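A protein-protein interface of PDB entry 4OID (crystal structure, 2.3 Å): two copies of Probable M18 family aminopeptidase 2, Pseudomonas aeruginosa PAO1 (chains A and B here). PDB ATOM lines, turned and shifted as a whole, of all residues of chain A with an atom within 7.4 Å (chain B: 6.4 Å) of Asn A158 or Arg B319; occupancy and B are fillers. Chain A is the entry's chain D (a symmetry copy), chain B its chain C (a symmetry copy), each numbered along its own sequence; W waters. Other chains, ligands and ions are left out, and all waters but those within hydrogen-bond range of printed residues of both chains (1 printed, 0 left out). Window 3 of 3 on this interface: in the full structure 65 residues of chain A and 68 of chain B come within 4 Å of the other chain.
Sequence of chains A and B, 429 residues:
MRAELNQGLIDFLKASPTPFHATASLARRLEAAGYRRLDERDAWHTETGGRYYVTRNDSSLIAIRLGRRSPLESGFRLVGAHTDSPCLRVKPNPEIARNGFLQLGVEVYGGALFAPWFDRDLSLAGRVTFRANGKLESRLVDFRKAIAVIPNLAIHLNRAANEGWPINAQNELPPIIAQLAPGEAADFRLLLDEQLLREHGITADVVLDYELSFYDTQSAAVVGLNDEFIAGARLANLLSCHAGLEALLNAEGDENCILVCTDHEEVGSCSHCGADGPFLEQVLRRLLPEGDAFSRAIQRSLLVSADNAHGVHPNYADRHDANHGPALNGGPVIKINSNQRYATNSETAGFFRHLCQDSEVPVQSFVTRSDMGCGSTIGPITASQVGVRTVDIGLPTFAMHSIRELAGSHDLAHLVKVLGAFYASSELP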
ATOM      1  N   ASN A 152       2.999 -13.645 -26.994  1.00  0.00           N
ATOM      2  CA  ASN A 152       2.445 -12.414 -26.439  1.00  0.00           C
ATOM      3  C   ASN A 152       1.870 -11.482 -27.525  1.00  0.00           C
ATOM      4  O   ASN A 152       2.283 -11.527 -28.711  1.00  0.00           O
ATOM      5  CB  ASN A 152       3.506 -11.596 -25.663  1.00  0.00           C
ATOM      6  CG  ASN A 152       3.508 -11.902 -24.171  1.00  0.00           C
ATOM      7  OD1 ASN A 152       2.486 -11.728 -23.509  1.00  0.00           O
ATOM      8  ND2 ASN A 152       4.661 -12.311 -23.632  1.00  0.00           N
ATOM      9  N   LEU A 153       0.907 -10.674 -27.111  1.00  0.00           N
ATOM     10  CA  LEU A 153       0.522  -9.437 -27.861  1.00  0.00           C
ATOM     11  C   LEU A 153       1.599  -8.331 -27.754  1.00  0.00           C
ATOM     12  O   LEU A 153       2.062  -7.979 -26.638  1.00  0.00           O
ATOM     13  CB  LEU A 153      -0.811  -8.879 -27.385  1.00  0.00           C
ATOM     14  CG  LEU A 153      -1.313  -7.657 -28.191  1.00  0.00           C
ATOM     15  CD1 LEU A 153      -1.394  -7.986 -29.673  1.00  0.00           C
ATOM     16  CD2 LEU A 153      -2.685  -7.122 -27.635  1.00  0.00           C
ATOM     17  N   ALA A 154       2.015  -7.806 -28.915  1.00  0.00           N
ATOM     18  CA  ALA A 154       3.040  -6.760 -28.942  1.00  0.00           C
ATOM     19  C   ALA A 154       2.597  -5.567 -28.065  1.00  0.00           C
ATOM     20  O   ALA A 154       1.377  -5.289 -27.904  1.00  0.00           O
ATOM     21  CB  ALA A 154       3.336  -6.314 -30.365  1.00  0.00           C
ATOM     22  N   ILE A 155       3.594  -4.912 -27.461  1.00  0.00           N
ATOM     23  CA  ILE A 155       3.351  -3.818 -26.512  1.00  0.00           C
ATOM     24  C   ILE A 155       2.773  -2.590 -27.264  1.00  0.00           C
ATOM     25  O   ILE A 155       1.875  -1.924 -26.766  1.00  0.00           O
ATOM     26  CB  ILE A 155       4.634  -3.468 -25.674  1.00  0.00           C
ATOM     27  CG1 ILE A 155       4.250  -2.522 -24.486  1.00  0.00           C
ATOM     28  CG2 ILE A 155       5.747  -2.932 -26.598  1.00  0.00           C
ATOM     29  CD1 ILE A 155       5.351  -2.240 -23.446  1.00  0.00           C
ATOM     30  N   HIS A 156       3.265  -2.329 -28.481  1.00  0.00           N
ATOM     31  CA  HIS A 156       2.647  -1.332 -29.414  1.00  0.00           C
ATOM     32  C   HIS A 156       1.098  -1.434 -29.488  1.00  0.00           C
ATOM     33  O   HIS A 156       0.435  -0.405 -29.658  1.00  0.00           O
ATOM     34  CB  HIS A 156       3.180  -1.480 -30.848  1.00  0.00           C
ATOM     35  CG  HIS A 156       4.672  -1.588 -30.944  1.00  0.00           C
ATOM     36  ND1 HIS A 156       5.378  -2.632 -30.378  1.00  0.00           N
ATOM     37  CD2 HIS A 156       5.587  -0.805 -31.568  1.00  0.00           C
ATOM     38  CE1 HIS A 156       6.666  -2.472 -30.621  1.00  0.00           C
ATOM     39  NE2 HIS A 156       6.820  -1.375 -31.351  1.00  0.00           N
ATOM     40  N   LEU A 157       0.562  -2.671 -29.373  1.00  0.00           N
ATOM     41  CA  LEU A 157      -0.879  -2.962 -29.443  1.00  0.00           C
ATOM     42  C   LEU A 157      -1.537  -3.374 -28.066  1.00  0.00           C
ATOM     43  O   LEU A 157      -2.725  -3.734 -27.991  1.00  0.00           O
ATOM     44  CB  LEU A 157      -1.115  -4.036 -30.531  1.00  0.00           C
ATOM     45  CG  LEU A 157      -0.791  -3.646 -31.988  1.00  0.00           C
ATOM     46  CD1 LEU A 157      -0.669  -4.906 -32.839  1.00  0.00           C
ATOM     47  CD2 LEU A 157      -1.807  -2.646 -32.574  1.00  0.00           C
ATOM     48  N   ASN A 158      -0.726  -3.345 -27.017  1.00  0.00           N
ATOM     49  CA  ASN A 158      -1.138  -3.592 -25.642  1.00  0.00           C
ATOM     50  C   ASN A 158      -0.239  -2.665 -24.818  1.00  0.00           C
ATOM     51  O   ASN A 158       0.802  -3.072 -24.271  1.00  0.00           O
ATOM     52  CB  ASN A 158      -0.938  -5.074 -25.262  1.00  0.00           C
ATOM     53  CG  ASN A 158      -1.407  -5.393 -23.851  1.00  0.00           C
ATOM     54  OD1 ASN A 158      -2.159  -4.619 -23.236  1.00  0.00           O
ATOM     55  ND2 ASN A 158      -0.988  -6.557 -23.337  1.00  0.00           N
ATOM     56  N   ARG A 159      -0.632  -1.398 -24.786  1.00  0.00           N
ATOM     57  CA  ARG A 159       0.243  -0.321 -24.308  1.00  0.00           C
ATOM     58  C   ARG A 159       0.579  -0.532 -22.818  1.00  0.00           C
ATOM     59  O   ARG A 159       1.765  -0.559 -22.422  1.00  0.00           O
ATOM     60  CB  ARG A 159      -0.433   1.051 -24.533  1.00  0.00           C
ATOM     61  CG  ARG A 159      -1.066   1.286 -25.916  1.00  0.00           C
ATOM     62  CD  ARG A 159      -0.112   0.996 -27.080  1.00  0.00           C
ATOM     63  NE  ARG A 159       1.234   1.561 -26.894  1.00  0.00           N
ATOM     64  CZ  ARG A 159       1.595   2.823 -27.155  1.00  0.00           C
ATOM     65  NH1 ARG A 159       0.717   3.702 -27.629  1.00  0.00           N
ATOM     66  NH2 ARG A 159       2.851   3.214 -26.925  1.00  0.00           N
ATOM     67  N   ALA A 160      -0.486  -0.723 -22.026  1.00  0.00           N
ATOM     68  CA  ALA A 160      -0.405  -0.941 -20.586  1.00  0.00           C
ATOM     69  C   ALA A 160      -0.149  -2.441 -20.245  1.00  0.00           C
ATOM     70  O   ALA A 160      -0.640  -2.973 -19.236  1.00  0.00           O
ATOM     71  CB  ALA A 160      -1.679  -0.404 -19.909  1.00  0.00           C
ATOM     72  N   ALA A 161       0.627  -3.109 -21.094  1.00  0.00           N
ATOM     73  CA  ALA A 161       1.051  -4.508 -20.862  1.00  0.00           C
ATOM     74  C   ALA A 161       1.707  -4.617 -19.498  1.00  0.00           C
ATOM     75  O   ALA A 161       1.384  -5.516 -18.704  1.00  0.00           O
ATOM     76  CB  ALA A 161       2.039  -4.975 -21.946  1.00  0.00           C
ATOM     77  N   ASN A 162       2.612  -3.670 -19.235  1.00  0.00           N
ATOM     78  CA  ASN A 162       3.423  -3.688 -18.014  1.00  0.00           C
ATOM     79  C   ASN A 162       2.697  -3.307 -16.709  1.00  0.00           C
ATOM     80  O   ASN A 162       3.223  -3.576 -15.653  1.00  0.00           O
ATOM     81  CB  ASN A 162       4.731  -2.911 -18.231  1.00  0.00           C
ATOM     82  CG  ASN A 162       5.641  -3.594 -19.281  1.00  0.00           C
ATOM     83  OD1 ASN A 162       5.664  -4.822 -19.405  1.00  0.00           O
ATOM     84  ND2 ASN A 162       6.372  -2.793 -20.044  1.00  0.00           N
ATOM     85  N   GLY A 164      -0.096  -4.831 -15.887  1.00  0.00           N
ATOM     86  CA  GLY A 164      -0.815  -6.052 -15.586  1.00  0.00           C
ATOM     87  C   GLY A 164      -2.120  -6.042 -16.360  1.00  0.00           C
ATOM     88  O   GLY A 164      -2.649  -4.977 -16.649  1.00  0.00           O
ATOM     89  N   TRP A 165      -2.599  -7.228 -16.743  1.00  0.00           N
ATOM     90  CA  TRP A 165      -4.010  -7.448 -17.159  1.00  0.00           C
ATOM     91  C   TRP A 165      -4.447  -8.890 -16.756  1.00  0.00           C
ATOM     92  O   TRP A 165      -3.584  -9.775 -16.618  1.00  0.00           O
ATOM     93  CB  TRP A 165      -4.241  -7.190 -18.675  1.00  0.00           C
ATOM     94  CG  TRP A 165      -3.671  -8.256 -19.606  1.00  0.00           C
ATOM     95  CD1 TRP A 165      -4.360  -9.303 -20.191  1.00  0.00           C
ATOM     96  CD2 TRP A 165      -2.298  -8.371 -20.061  1.00  0.00           C
ATOM     97  NE1 TRP A 165      -3.499 -10.063 -20.977  1.00  0.00           N
ATOM     98  CE2 TRP A 165      -2.233  -9.522 -20.911  1.00  0.00           C
ATOM     99  CE3 TRP A 165      -1.128  -7.624 -19.830  1.00  0.00           C
ATOM    100  CZ2 TRP A 165      -1.030  -9.932 -21.545  1.00  0.00           C
ATOM    101  CZ3 TRP A 165       0.073  -8.032 -20.451  1.00  0.00           C
ATOM    102  CH2 TRP A 165       0.107  -9.178 -21.305  1.00  0.00           C
ATOM    103  N   GLU A 172      -6.452 -16.644 -24.664  1.00  0.00           N
ATOM    104  CA  GLU A 172      -5.122 -16.180 -24.884  1.00  0.00           C
ATOM    105  C   GLU A 172      -4.145 -17.264 -24.871  1.00  0.00           C
ATOM    106  O   GLU A 172      -3.079 -17.070 -25.364  1.00  0.00           O
ATOM    107  CB  GLU A 172      -4.761 -15.131 -23.812  1.00  0.00           C
ATOM    108  CG  GLU A 172      -5.546 -13.824 -24.008  1.00  0.00           C
ATOM    109  CD  GLU A 172      -5.261 -12.770 -22.943  1.00  0.00           C
ATOM    110  OE1 GLU A 172      -6.219 -12.350 -22.294  1.00  0.00           O
ATOM    111  OE2 GLU A 172      -4.080 -12.380 -22.769  1.00  0.00           O
ATOM    112  N   LEU B 113       8.639  -5.235 -23.220  1.00  0.00           N
ATOM    113  CA  LEU B 113       7.662  -5.985 -22.398  1.00  0.00           C
ATOM    114  C   LEU B 113       8.394  -6.618 -21.180  1.00  0.00           C
ATOM    115  O   LEU B 113       9.334  -7.435 -21.360  1.00  0.00           O
ATOM    116  CB  LEU B 113       7.080  -7.127 -23.217  1.00  0.00           C
ATOM    117  CG  LEU B 113       6.133  -6.764 -24.338  1.00  0.00           C
ATOM    118  CD1 LEU B 113       6.143  -7.796 -25.471  1.00  0.00           C
ATOM    119  CD2 LEU B 113       4.734  -6.612 -23.746  1.00  0.00           C
ATOM    120  N   VAL B 312      -1.665  -9.886 -37.591  1.00  0.00           N
ATOM    121  CA  VAL B 312      -2.928 -10.125 -36.848  1.00  0.00           C
ATOM    122  C   VAL B 312      -2.832 -11.412 -35.989  1.00  0.00           C
ATOM    123  O   VAL B 312      -2.557 -12.509 -36.488  1.00  0.00           O
ATOM    124  CB  VAL B 312      -4.178 -10.153 -37.771  1.00  0.00           C
ATOM    125  CG1 VAL B 312      -4.127 -11.371 -38.719  1.00  0.00           C
ATOM    126  CG2 VAL B 312      -5.465 -10.139 -36.933  1.00  0.00           C
ATOM    127  N   TYR B 316      -5.866 -12.404 -30.334  1.00  0.00           N
ATOM    128  CA  TYR B 316      -6.095 -10.988 -30.083  1.00  0.00           C
ATOM    129  C   TYR B 316      -6.379 -10.267 -31.430  1.00  0.00           C
ATOM    130  O   TYR B 316      -5.727  -9.240 -31.762  1.00  0.00           O
ATOM    131  CB  TYR B 316      -4.874 -10.308 -29.399  1.00  0.00           C
ATOM    132  CG  TYR B 316      -4.241 -10.934 -28.136  1.00  0.00           C
ATOM    133  CD1 TYR B 316      -3.180 -11.875 -28.227  1.00  0.00           C
ATOM    134  CD2 TYR B 316      -4.628 -10.498 -26.856  1.00  0.00           C
ATOM    135  CE1 TYR B 316      -2.576 -12.390 -27.067  1.00  0.00           C
ATOM    136  CE2 TYR B 316      -4.029 -10.993 -25.702  1.00  0.00           C
ATOM    137  CZ  TYR B 316      -3.011 -11.944 -25.784  1.00  0.00           C
ATOM    138  OH  TYR B 316      -2.448 -12.412 -24.586  1.00  0.00           O
ATOM    139  N   ALA B 317      -7.333 -10.813 -32.198  1.00  0.00           N
ATOM    140  CA  ALA B 317      -7.528 -10.419 -33.595  1.00  0.00           C
ATOM    141  C   ALA B 317      -8.116  -9.025 -33.675  1.00  0.00           C
ATOM    142  O   ALA B 317      -7.715  -8.221 -34.524  1.00  0.00           O
ATOM    143  CB  ALA B 317      -8.384 -11.445 -34.368  1.00  0.00           C
ATOM    144  N   ASP B 318      -9.062  -8.725 -32.785  1.00  0.00           N
ATOM    145  CA  ASP B 318      -9.741  -7.431 -32.838  1.00  0.00           C
ATOM    146  C   ASP B 318      -8.764  -6.243 -32.517  1.00  0.00           C
ATOM    147  O   ASP B 318      -9.096  -5.083 -32.737  1.00  0.00           O
ATOM    148  CB  ASP B 318     -11.054  -7.462 -32.029  1.00  0.00           C
ATOM    149  CG  ASP B 318     -10.883  -7.036 -30.588  1.00  0.00           C
ATOM    150  OD1 ASP B 318      -9.945  -7.550 -29.933  1.00  0.00           O
ATOM    151  OD2 ASP B 318     -11.709  -6.192 -30.114  1.00  0.00           O
ATOM    152  N   ARG B 319      -7.539  -6.552 -32.081  1.00  0.00           N
ATOM    153  CA  ARG B 319      -6.472  -5.548 -31.992  1.00  0.00           C
ATOM    154  C   ARG B 319      -5.931  -5.049 -33.361  1.00  0.00           C
ATOM    155  O   ARG B 319      -5.129  -4.092 -33.397  1.00  0.00           O
ATOM    156  CB  ARG B 319      -5.316  -6.072 -31.126  1.00  0.00           C
ATOM    157  CG  ARG B 319      -5.717  -6.433 -29.698  1.00  0.00           C
ATOM    158  CD  ARG B 319      -6.000  -5.206 -28.837  1.00  0.00           C
ATOM    159  NE  ARG B 319      -6.166  -5.595 -27.431  1.00  0.00           N
ATOM    160  CZ  ARG B 319      -5.498  -5.090 -26.384  1.00  0.00           C
ATOM    161  NH1 ARG B 319      -4.600  -4.114 -26.521  1.00  0.00           N
ATOM    162  NH2 ARG B 319      -5.750  -5.560 -25.163  1.00  0.00           N
ATOM    163  N   HIS B 320      -6.366  -5.701 -34.452  1.00  0.00           N
ATOM    164  CA  HIS B 320      -6.144  -5.245 -35.863  1.00  0.00           C
ATOM    165  C   HIS B 320      -7.417  -4.702 -36.546  1.00  0.00           C
ATOM    166  O   HIS B 320      -8.526  -4.980 -36.102  1.00  0.00           O
ATOM    167  CB  HIS B 320      -5.538  -6.382 -36.730  1.00  0.00           C
ATOM    168  CG  HIS B 320      -4.038  -6.461 -36.640  1.00  0.00           C
ATOM    169  ND1 HIS B 320      -3.383  -6.990 -35.545  1.00  0.00           N
ATOM    170  CD2 HIS B 320      -3.068  -6.018 -37.473  1.00  0.00           C
ATOM    171  CE1 HIS B 320      -2.081  -6.911 -35.730  1.00  0.00           C
ATOM    172  NE2 HIS B 320      -1.862  -6.321 -36.889  1.00  0.00           N
ATOM    173  N   ASP B 321      -7.222  -3.893 -37.598  1.00  0.00           N
ATOM    174  CA  ASP B 321      -8.254  -3.609 -38.605  1.00  0.00           C
ATOM    175  C   ASP B 321      -8.489  -4.947 -39.378  1.00  0.00           C
ATOM    176  O   ASP B 321      -7.543  -5.510 -39.981  1.00  0.00           O
ATOM    177  CB  ASP B 321      -7.815  -2.454 -39.554  1.00  0.00           C
ATOM    178  CG  ASP B 321      -8.933  -2.037 -40.580  1.00  0.00           C
ATOM    179  OD1 ASP B 321      -9.194  -2.806 -41.556  1.00  0.00           O
ATOM    180  OD2 ASP B 321      -9.530  -0.923 -40.422  1.00  0.00           O
ATOM    181  N   PHE B 366      -0.998  -2.364 -44.061  1.00  0.00           N
ATOM    182  CA  PHE B 366      -1.307  -2.187 -42.644  1.00  0.00           C
ATOM    183  C   PHE B 366      -1.349  -0.681 -42.471  1.00  0.00           C
ATOM    184  O   PHE B 366      -0.467   0.041 -42.929  1.00  0.00           O
ATOM    185  CB  PHE B 366      -0.242  -2.827 -41.681  1.00  0.00           C
ATOM    186  CG  PHE B 366      -0.361  -2.370 -40.207  1.00  0.00           C
ATOM    187  CD1 PHE B 366       0.305  -1.216 -39.737  1.00  0.00           C
ATOM    188  CD2 PHE B 366      -1.162  -3.087 -39.280  1.00  0.00           C
ATOM    189  CE1 PHE B 366       0.147  -0.793 -38.415  1.00  0.00           C
ATOM    190  CE2 PHE B 366      -1.314  -2.662 -37.946  1.00  0.00           C
ATOM    191  CZ  PHE B 366      -0.651  -1.528 -37.513  1.00  0.00           C
ATOM    192  N   ARG B 369      -5.414   0.481 -36.326  1.00  0.00           N
ATOM    193  CA  ARG B 369      -6.864   0.721 -36.137  1.00  0.00           C
ATOM    194  C   ARG B 369      -7.058   2.213 -35.848  1.00  0.00           C
ATOM    195  O   ARG B 369      -6.196   2.840 -35.175  1.00  0.00           O
ATOM    196  CB  ARG B 369      -7.461  -0.095 -34.995  1.00  0.00           C
ATOM    197  CG  ARG B 369      -7.781  -1.545 -35.324  1.00  0.00           C
ATOM    198  CD  ARG B 369      -8.154  -2.305 -34.055  1.00  0.00           C
ATOM    199  NE  ARG B 369      -9.354  -1.795 -33.379  1.00  0.00           N
ATOM    200  CZ  ARG B 369     -10.606  -2.092 -33.735  1.00  0.00           C
ATOM    201  NH1 ARG B 369     -10.830  -2.874 -34.793  1.00  0.00           N
ATOM    202  NH2 ARG B 369     -11.637  -1.582 -33.053  1.00  0.00           N
ATOM    203  N   MET B 372      -6.850   3.661 -32.283  1.00  0.00           N
ATOM    204  CA  MET B 372      -5.606   3.235 -31.591  1.00  0.00           C
ATOM    205  C   MET B 372      -4.420   4.131 -31.972  1.00  0.00           C
ATOM    206  O   MET B 372      -4.355   5.302 -31.598  1.00  0.00           O
ATOM    207  CB  MET B 372      -5.282   1.761 -31.954  1.00  0.00           C
ATOM    208  CG  MET B 372      -5.140   0.796 -30.774  1.00  0.00           C
ATOM    209  SD  MET B 372      -5.524  -0.942 -31.152  1.00  0.00           S
ATOM    210  CE  MET B 372      -5.740  -1.589 -29.488  1.00  0.00           C
HETATM  211  O   HOH W   1       0.085 -11.171 -24.305  1.00  0.00           O
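The guanidinium group (NH1) of Arg B369 sits at hydrogen-bond distance from the backbone carbonyl oxygen (O) of His B320 (3.4 Å). The side-chain carboxylate of Glu A172 lies within hydrogen-bond range of the indole nitrogen of Trp A165, 3.0 Å away.
No position is printed for both chains.
Among the printed residues, pairs that only touch across the chains: Leu A153 with Tyr B316 (3.9 Å), Leu A153 with Arg B319 (3.7 Å), Ile A155 with Leu B113 (3.7 Å), Leu A157 with His B320 (3.8 Å), Leu A157 with Met B372 (3.99 Å), Asn A158 with Arg B319 (3.6 Å), Ala A161 with Leu B113 (3.6 Å) and Asn A162 with Leu B113 (3.7 Å).
OE2 of Glu A172 lies within hydrogen-bond range of OH of Tyr B316. The backbone carbonyl oxygen of Leu A157 sits at hydrogen-bond distance from the guanidinium group of Arg B319 (2.4 Å).
Of the 11 printed residues of chain B, 5 touch a printed residue of chain A. Hydrophobic or aromatic side chains of chain B within 4 Å of the printed part of chain A: Leu B113, Tyr B316, His B320 and Met B372. Of the 14 printed residues of chain A, 7 touch a printed residue of chain B. Printed residues of chain A that touch a printed residue of chain B: Leu A153, Ile A155, Leu A157, Asn A158, Ala A161, Asn A162 and Glu A172. Hydrophobic or aromatic side chains of chain A that line the printed part of chain B: Leu A153, Ile A155, Leu A157 and Ala A161. Among the printed residues, 10 pairs touch across the chains.
Asn A158 touches just one residue of chain B: Arg B319 (3.6 Å). Arg B319 touches just these residues of chain A: Leu A153, Leu A157 and Asn A158. Of the printed residues of chain A, His B320 touches Leu A157 (3.8 Å). Of the printed residues of chain B, Glu A172 touches Tyr B316. Printed residues of chain B within 4 Å of Leu A153: Tyr B316 (3.9 Å) and Arg B319 (3.7 Å). Of the printed residues of chain B, Asn A162 touches Leu B113 (3.7 Å). Asp B321 touches none of the printed residues of chain A. Asn A152 touches none of the printed residues of chain B. The nearest residue of chain B that does not touch Asn A158 is Leu B113 (5.3 Å). The nearest residue of chain A that does not touch Arg B319 is Arg A159 (5.1 Å).
Water W1 lies within hydrogen-bond range of OD1 of Asn A152, OH of Tyr B316 and N of Leu A153.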
